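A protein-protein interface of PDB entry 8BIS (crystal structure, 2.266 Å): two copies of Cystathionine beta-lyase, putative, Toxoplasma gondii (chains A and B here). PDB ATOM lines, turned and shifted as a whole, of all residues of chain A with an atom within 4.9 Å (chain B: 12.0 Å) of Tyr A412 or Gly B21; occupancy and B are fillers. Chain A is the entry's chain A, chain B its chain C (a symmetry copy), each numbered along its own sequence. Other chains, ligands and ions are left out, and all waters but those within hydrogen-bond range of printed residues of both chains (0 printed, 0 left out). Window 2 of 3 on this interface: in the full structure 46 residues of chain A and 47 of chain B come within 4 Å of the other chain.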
ATOM      1  N   HIS A 350       5.539   0.066   9.886  1.00  0.00           N
ATOM      2  CA  HIS A 350       5.551  -0.930   8.821  1.00  0.00           C
ATOM      3  C   HIS A 350       6.076  -2.283   9.285  1.00  0.00           C
ATOM      4  O   HIS A 350       6.433  -3.119   8.449  1.00  0.00           O
ATOM      5  CB  HIS A 350       6.375  -0.425   7.635  1.00  0.00           C
ATOM      6  CG  HIS A 350       5.786   0.773   6.962  1.00  0.00           C
ATOM      7  ND1 HIS A 350       6.275   2.048   7.155  1.00  0.00           N
ATOM      8  CD2 HIS A 350       4.742   0.894   6.110  1.00  0.00           C
ATOM      9  CE1 HIS A 350       5.559   2.901   6.444  1.00  0.00           C
ATOM     10  NE2 HIS A 350       4.622   2.227   5.801  1.00  0.00           N
ATOM     11  N   PRO A 352       5.294  -5.826  10.402  1.00  0.00           N
ATOM     12  CA  PRO A 352       4.066  -6.608  10.243  1.00  0.00           C
ATOM     13  C   PRO A 352       3.937  -7.681  11.317  1.00  0.00           C
ATOM     14  O   PRO A 352       4.846  -7.916  12.115  1.00  0.00           O
ATOM     15  CB  PRO A 352       4.254  -7.240   8.858  1.00  0.00           C
ATOM     16  CG  PRO A 352       5.729  -7.458   8.773  1.00  0.00           C
ATOM     17  CD  PRO A 352       6.387  -6.347   9.565  1.00  0.00           C
ATOM     18  N   ASP A 408      11.788 -12.149   8.959  1.00  0.00           N
ATOM     19  CA  ASP A 408      11.166 -11.613   7.751  1.00  0.00           C
ATOM     20  C   ASP A 408      10.427 -10.312   8.041  1.00  0.00           C
ATOM     21  O   ASP A 408      10.509  -9.354   7.261  1.00  0.00           O
ATOM     22  CB  ASP A 408      10.211 -12.639   7.138  1.00  0.00           C
ATOM     23  CG  ASP A 408      10.911 -13.914   6.708  1.00  0.00           C
ATOM     24  OD1 ASP A 408      10.232 -14.960   6.611  1.00  0.00           O
ATOM     25  OD2 ASP A 408      12.138 -13.876   6.477  1.00  0.00           O
ATOM     26  N   GLY A 409       9.689 -10.261   9.154  1.00  0.00           N
ATOM     27  CA  GLY A 409       9.001  -9.028   9.505  1.00  0.00           C
ATOM     28  C   GLY A 409       9.959  -7.870   9.716  1.00  0.00           C
ATOM     29  O   GLY A 409       9.753  -6.769   9.191  1.00  0.00           O
ATOM     30  N   LEU A 410      11.021  -8.104  10.494  1.00  0.00           N
ATOM     31  CA  LEU A 410      12.025  -7.068  10.721  1.00  0.00           C
ATOM     32  C   LEU A 410      12.667  -6.621   9.416  1.00  0.00           C
ATOM     33  O   LEU A 410      12.920  -5.428   9.215  1.00  0.00           O
ATOM     34  CB  LEU A 410      13.097  -7.574  11.681  1.00  0.00           C
ATOM     35  CG  LEU A 410      12.696  -7.650  13.145  1.00  0.00           C
ATOM     36  CD1 LEU A 410      13.817  -8.270  13.947  1.00  0.00           C
ATOM     37  CD2 LEU A 410      12.360  -6.263  13.662  1.00  0.00           C
ATOM     38  N   ASP A 411      12.943  -7.567   8.520  1.00  0.00           N
ATOM     39  CA  ASP A 411      13.592  -7.235   7.259  1.00  0.00           C
ATOM     40  C   ASP A 411      12.688  -6.376   6.387  1.00  0.00           C
ATOM     41  O   ASP A 411      13.151  -5.413   5.768  1.00  0.00           O
ATOM     42  CB  ASP A 411      13.992  -8.518   6.533  1.00  0.00           C
ATOM     43  CG  ASP A 411      14.903  -8.265   5.355  1.00  0.00           C
ATOM     44  OD1 ASP A 411      15.928  -7.572   5.527  1.00  0.00           O
ATOM     45  OD2 ASP A 411      14.594  -8.769   4.258  1.00  0.00           O
ATOM     46  N   TYR A 412      11.392  -6.692   6.344  1.00  0.00           N
ATOM     47  CA  TYR A 412      10.468  -5.855   5.582  1.00  0.00           C
ATOM     48  C   TYR A 412      10.365  -4.460   6.191  1.00  0.00           C
ATOM     49  O   TYR A 412      10.364  -3.446   5.474  1.00  0.00           O
ATOM     50  CB  TYR A 412       9.089  -6.511   5.510  1.00  0.00           C
ATOM     51  CG  TYR A 412       8.046  -5.607   4.891  1.00  0.00           C
ATOM     52  CD1 TYR A 412       8.002  -5.404   3.517  1.00  0.00           C
ATOM     53  CD2 TYR A 412       7.123  -4.933   5.682  1.00  0.00           C
ATOM     54  CE1 TYR A 412       7.059  -4.565   2.947  1.00  0.00           C
ATOM     55  CE2 TYR A 412       6.178  -4.090   5.121  1.00  0.00           C
ATOM     56  CZ  TYR A 412       6.151  -3.913   3.753  1.00  0.00           C
ATOM     57  OH  TYR A 412       5.216  -3.078   3.185  1.00  0.00           O
ATOM     58  N   ALA A 413      10.268  -4.391   7.522  1.00  0.00           N
ATOM     59  CA  ALA A 413      10.161  -3.094   8.182  1.00  0.00           C
ATOM     60  C   ALA A 413      11.397  -2.242   7.919  1.00  0.00           C
ATOM     61  O   ALA A 413      11.289  -1.034   7.673  1.00  0.00           O
ATOM     62  CB  ALA A 413       9.941  -3.289   9.683  1.00  0.00           C
ATOM     63  N   LEU A 414      12.582  -2.860   7.951  1.00  0.00           N
ATOM     64  CA  LEU A 414      13.812  -2.147   7.625  1.00  0.00           C
ATOM     65  C   LEU A 414      13.850  -1.746   6.157  1.00  0.00           C
ATOM     66  O   LEU A 414      14.425  -0.703   5.811  1.00  0.00           O
ATOM     67  CB  LEU A 414      15.021  -3.017   7.965  1.00  0.00           C
ATOM     68  CG  LEU A 414      15.429  -3.092   9.440  1.00  0.00           C
ATOM     69  CD1 LEU A 414      16.405  -4.231   9.650  1.00  0.00           C
ATOM     70  CD2 LEU A 414      16.027  -1.782   9.930  1.00  0.00           C
ATOM     71  N   SER A 415      13.263  -2.571   5.284  1.00  0.00           N
ATOM     72  CA  SER A 415      13.073  -2.170   3.901  1.00  0.00           C
ATOM     73  C   SER A 415      12.288  -0.871   3.803  1.00  0.00           C
ATOM     74  O   SER A 415      12.578  -0.025   2.952  1.00  0.00           O
ATOM     75  CB  SER A 415      12.360  -3.291   3.153  1.00  0.00           C
ATOM     76  OG  SER A 415      11.507  -2.798   2.144  1.00  0.00           O
ATOM     77  N   LYS A 416      11.282  -0.698   4.647  1.00  0.00           N
ATOM     78  CA  LYS A 416      10.489   0.525   4.579  1.00  0.00           C
ATOM     79  C   LYS A 416      11.164   1.724   5.234  1.00  0.00           C
ATOM     80  O   LYS A 416      10.661   2.842   5.090  1.00  0.00           O
ATOM     81  CB  LYS A 416       9.102   0.314   5.211  1.00  0.00           C
ATOM     82  CG  LYS A 416       8.148  -0.482   4.340  1.00  0.00           C
ATOM     83  CD  LYS A 416       8.503  -0.396   2.867  1.00  0.00           C
ATOM     84  CE  LYS A 416       7.286  -0.654   2.009  1.00  0.00           C
ATOM     85  NZ  LYS A 416       6.572   0.609   1.686  1.00  0.00           N
ATOM     86  N   GLY B  21       2.432  -3.072   0.193  1.00  0.00           N
ATOM     87  CA  GLY B  21       2.455  -1.945   1.107  1.00  0.00           C
ATOM     88  C   GLY B  21       1.687  -2.184   2.394  1.00  0.00           C
ATOM     89  O   GLY B  21       0.768  -1.432   2.725  1.00  0.00           O
ATOM     90  N   VAL B  22       2.064  -3.234   3.123  1.00  0.00           N
ATOM     91  CA  VAL B  22       1.392  -3.561   4.375  1.00  0.00           C
ATOM     92  C   VAL B  22       1.971  -2.721   5.509  1.00  0.00           C
ATOM     93  O   VAL B  22       3.102  -2.229   5.449  1.00  0.00           O
ATOM     94  CB  VAL B  22       1.495  -5.064   4.688  1.00  0.00           C
ATOM     95  CG1 VAL B  22       0.641  -5.863   3.716  1.00  0.00           C
ATOM     96  CG2 VAL B  22       2.944  -5.520   4.637  1.00  0.00           C
ATOM     97  N   LYS B  23       1.174  -2.553   6.558  1.00  0.00           N
ATOM     98  CA  LYS B  23       1.535  -1.759   7.722  1.00  0.00           C
ATOM     99  C   LYS B  23       1.456  -2.629   8.973  1.00  0.00           C
ATOM    100  O   LYS B  23       1.180  -3.829   8.906  1.00  0.00           O
ATOM    101  CB  LYS B  23       0.629  -0.530   7.841  1.00  0.00           C
ATOM    102  N   ALA B  24       1.713  -2.006  10.120  1.00  0.00           N
ATOM    103  CA  ALA B  24       1.647  -2.714  11.390  1.00  0.00           C
ATOM    104  C   ALA B  24       0.230  -3.207  11.649  1.00  0.00           C
ATOM    105  O   ALA B  24      -0.739  -2.455  11.505  1.00  0.00           O
ATOM    106  CB  ALA B  24       2.111  -1.803  12.527  1.00  0.00           C
ATOM    107  N   GLY B  25       0.111  -4.476  12.031  1.00  0.00           N
ATOM    108  CA  GLY B  25      -1.166  -5.127  12.195  1.00  0.00           C
ATOM    109  C   GLY B  25      -1.542  -6.056  11.060  1.00  0.00           C
ATOM    110  O   GLY B  25      -2.449  -6.879  11.224  1.00  0.00           O
ATOM    111  N   ASP B  26      -0.869  -5.952   9.920  1.00  0.00           N
ATOM    112  CA  ASP B  26      -1.108  -6.835   8.790  1.00  0.00           C
ATOM    113  C   ASP B  26      -0.031  -7.908   8.722  1.00  0.00           C
ATOM    114  O   ASP B  26       1.100  -7.709   9.170  1.00  0.00           O
ATOM    115  CB  ASP B  26      -1.136  -6.058   7.472  1.00  0.00           C
ATOM    116  CG  ASP B  26      -2.105  -4.893   7.498  1.00  0.00           C
ATOM    117  OD1 ASP B  26      -3.008  -4.884   8.363  1.00  0.00           O
ATOM    118  OD2 ASP B  26      -1.963  -3.991   6.646  1.00  0.00           O
ATOM    119  N   TRP B  27      -0.396  -9.054   8.162  1.00  0.00           N
ATOM    120  CA  TRP B  27       0.581 -10.082   7.851  1.00  0.00           C
ATOM    121  C   TRP B  27       1.120  -9.869   6.440  1.00  0.00           C
ATOM    122  O   TRP B  27       0.484  -9.231   5.598  1.00  0.00           O
ATOM    123  CB  TRP B  27      -0.032 -11.477   7.970  1.00  0.00           C
ATOM    124  CG  TRP B  27      -0.538 -11.812   9.339  1.00  0.00           C
ATOM    125  CD1 TRP B  27      -1.711 -11.400   9.903  1.00  0.00           C
ATOM    126  CD2 TRP B  27       0.103 -12.646  10.311  1.00  0.00           C
ATOM    127  NE1 TRP B  27      -1.835 -11.918  11.169  1.00  0.00           N
ATOM    128  CE2 TRP B  27      -0.734 -12.688  11.444  1.00  0.00           C
ATOM    129  CE3 TRP B  27       1.309 -13.356  10.337  1.00  0.00           C
ATOM    130  CZ2 TRP B  27      -0.405 -13.410  12.590  1.00  0.00           C
ATOM    131  CZ3 TRP B  27       1.634 -14.075  11.475  1.00  0.00           C
ATOM    132  CH2 TRP B  27       0.779 -14.096  12.586  1.00  0.00           C
ATOM    133  N   LEU B  28       2.303 -10.410   6.190  1.00  0.00           N
ATOM    134  CA  LEU B  28       2.885 -10.317   4.861  1.00  0.00           C
ATOM    135  C   LEU B  28       2.002 -11.060   3.864  1.00  0.00           C
ATOM    136  O   LEU B  28       1.652 -12.224   4.102  1.00  0.00           O
ATOM    137  CB  LEU B  28       4.297 -10.896   4.838  1.00  0.00           C
ATOM    138  CG  LEU B  28       5.383 -10.031   5.477  1.00  0.00           C
ATOM    139  CD1 LEU B  28       6.763 -10.606   5.187  1.00  0.00           C
ATOM    140  CD2 LEU B  28       5.275  -8.594   4.991  1.00  0.00           C
ATOM    141  N   PRO B  29       1.615 -10.432   2.757  1.00  0.00           N
ATOM    142  CA  PRO B  29       0.779 -11.129   1.770  1.00  0.00           C
ATOM    143  C   PRO B  29       1.538 -12.283   1.130  1.00  0.00           C
ATOM    144  O   PRO B  29       2.701 -12.144   0.749  1.00  0.00           O
ATOM    145  CB  PRO B  29       0.444 -10.032   0.751  1.00  0.00           C
ATOM    146  CG  PRO B  29       1.539  -9.023   0.911  1.00  0.00           C
ATOM    147  CD  PRO B  29       1.895  -9.041   2.365  1.00  0.00           C
ATOM    148  N   GLY B  30       0.869 -13.430   1.028  1.00  0.00           N
ATOM    149  CA  GLY B  30       1.457 -14.600   0.408  1.00  0.00           C
ATOM    150  C   GLY B  30       2.392 -15.399   1.285  1.00  0.00           C
ATOM    151  O   GLY B  30       3.120 -16.253   0.767  1.00  0.00           O
ATOM    152  N   PHE B  31       2.397 -15.158   2.592  1.00  0.00           N
ATOM    153  CA  PHE B  31       3.270 -15.854   3.528  1.00  0.00           C
ATOM    154  C   PHE B  31       2.428 -16.732   4.441  1.00  0.00           C
ATOM    155  O   PHE B  31       1.589 -16.223   5.191  1.00  0.00           O
ATOM    156  CB  PHE B  31       4.077 -14.864   4.364  1.00  0.00           C
ATOM    157  CG  PHE B  31       5.362 -14.447   3.733  1.00  0.00           C
ATOM    158  CD1 PHE B  31       6.558 -15.003   4.147  1.00  0.00           C
ATOM    159  CD2 PHE B  31       5.377 -13.491   2.730  1.00  0.00           C
ATOM    160  CE1 PHE B  31       7.749 -14.615   3.572  1.00  0.00           C
ATOM    161  CE2 PHE B  31       6.565 -13.096   2.152  1.00  0.00           C
ATOM    162  CZ  PHE B  31       7.753 -13.662   2.571  1.00  0.00           C
ATOM    163  N   ARG B  34       4.834 -19.688  10.039  1.00  0.00           N
ATOM    164  CA  ARG B  34       5.397 -20.963  10.444  1.00  0.00           C
ATOM    165  C   ARG B  34       4.634 -21.518  11.645  1.00  0.00           C
ATOM    166  O   ARG B  34       3.754 -20.867  12.212  1.00  0.00           O
ATOM    167  CB  ARG B  34       6.880 -20.813  10.761  1.00  0.00           C
ATOM    168  CG  ARG B  34       7.802 -20.761   9.554  1.00  0.00           C
ATOM    169  CD  ARG B  34       7.777 -19.392   8.890  1.00  0.00           C
ATOM    170  NE  ARG B  34       8.881 -19.206   7.955  1.00  0.00           N
ATOM    171  CZ  ARG B  34       9.085 -18.091   7.263  1.00  0.00           C
ATOM    172  NH1 ARG B  34       8.254 -17.067   7.396  1.00  0.00           N
ATOM    173  NH2 ARG B  34      10.116 -18.002   6.433  1.00  0.00           N
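OD1 of Asp A408 lies within salt-bridge range of NH1 of Arg B34, at 3.0 Å.
The side-chain hydroxyl of Tyr A412 sits at hydrogen-bond distance from the backbone NH of Val B22.
N of Lys B23 is in hydrogen-bond range of OD2 of Asp B26 (3.5 Å).
O of Val B22 touches CD2 of His A350, 3.6 Å away.
CB of Pro A352 touches O of Asp B26, at 3.2 Å.
Pro A352 touches Leu B28.
Asp A408 touches Phe B31.
Tyr A412 touches Gly B21 (OH to CA, 3.6 Å).
Tyr A412 touches just these residues of chain B: Gly B21 (3.6 Å) and Val B22 (3.2 Å).
Gly B21 touches just one residue of chain A: Tyr A412.
Of chain B, only Val B22 comes within 4 Å of His A350.
No residue of chain B comes within 4 Å of Gly A409.
No residue of chain B comes within 4 Å of Ala A413.
No residue of chain B comes within 4 Å of Leu A414.
No residue of chain B comes within 4 Å of Ser A415.
No residue of chain B comes within 4 Å of Lys A416.
Of the printed residues of chain A, Leu B28 touches Pro A352.
Of the printed residues of chain B, Asp A408 touches Phe B31 (3.9 Å) and Arg B34 (3.0 Å).
Of the printed residues of chain A, Asp B26 touches Pro A352.
The nearest residue of chain B that does not touch Tyr A412 is Leu B28 (4.1 Å).
Hydrophobic or aromatic side chains of chain B that line the printed part of chain A: Val B22, Leu B28 and Phe B31.
Of the 11 printed residues of chain A, 4 touch a printed residue of chain B.
Printed residues of chain A that touch a printed residue of chain B: His A350, Pro A352, Asp A408 and Tyr A412.
Hydrophobic or aromatic side chains of chain A within 4 Å of the printed part of chain B: His A350, Pro A352 and Tyr A412.
Among the printed residues, 7 pairs touch across the chains.
No position is printed for both chains.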
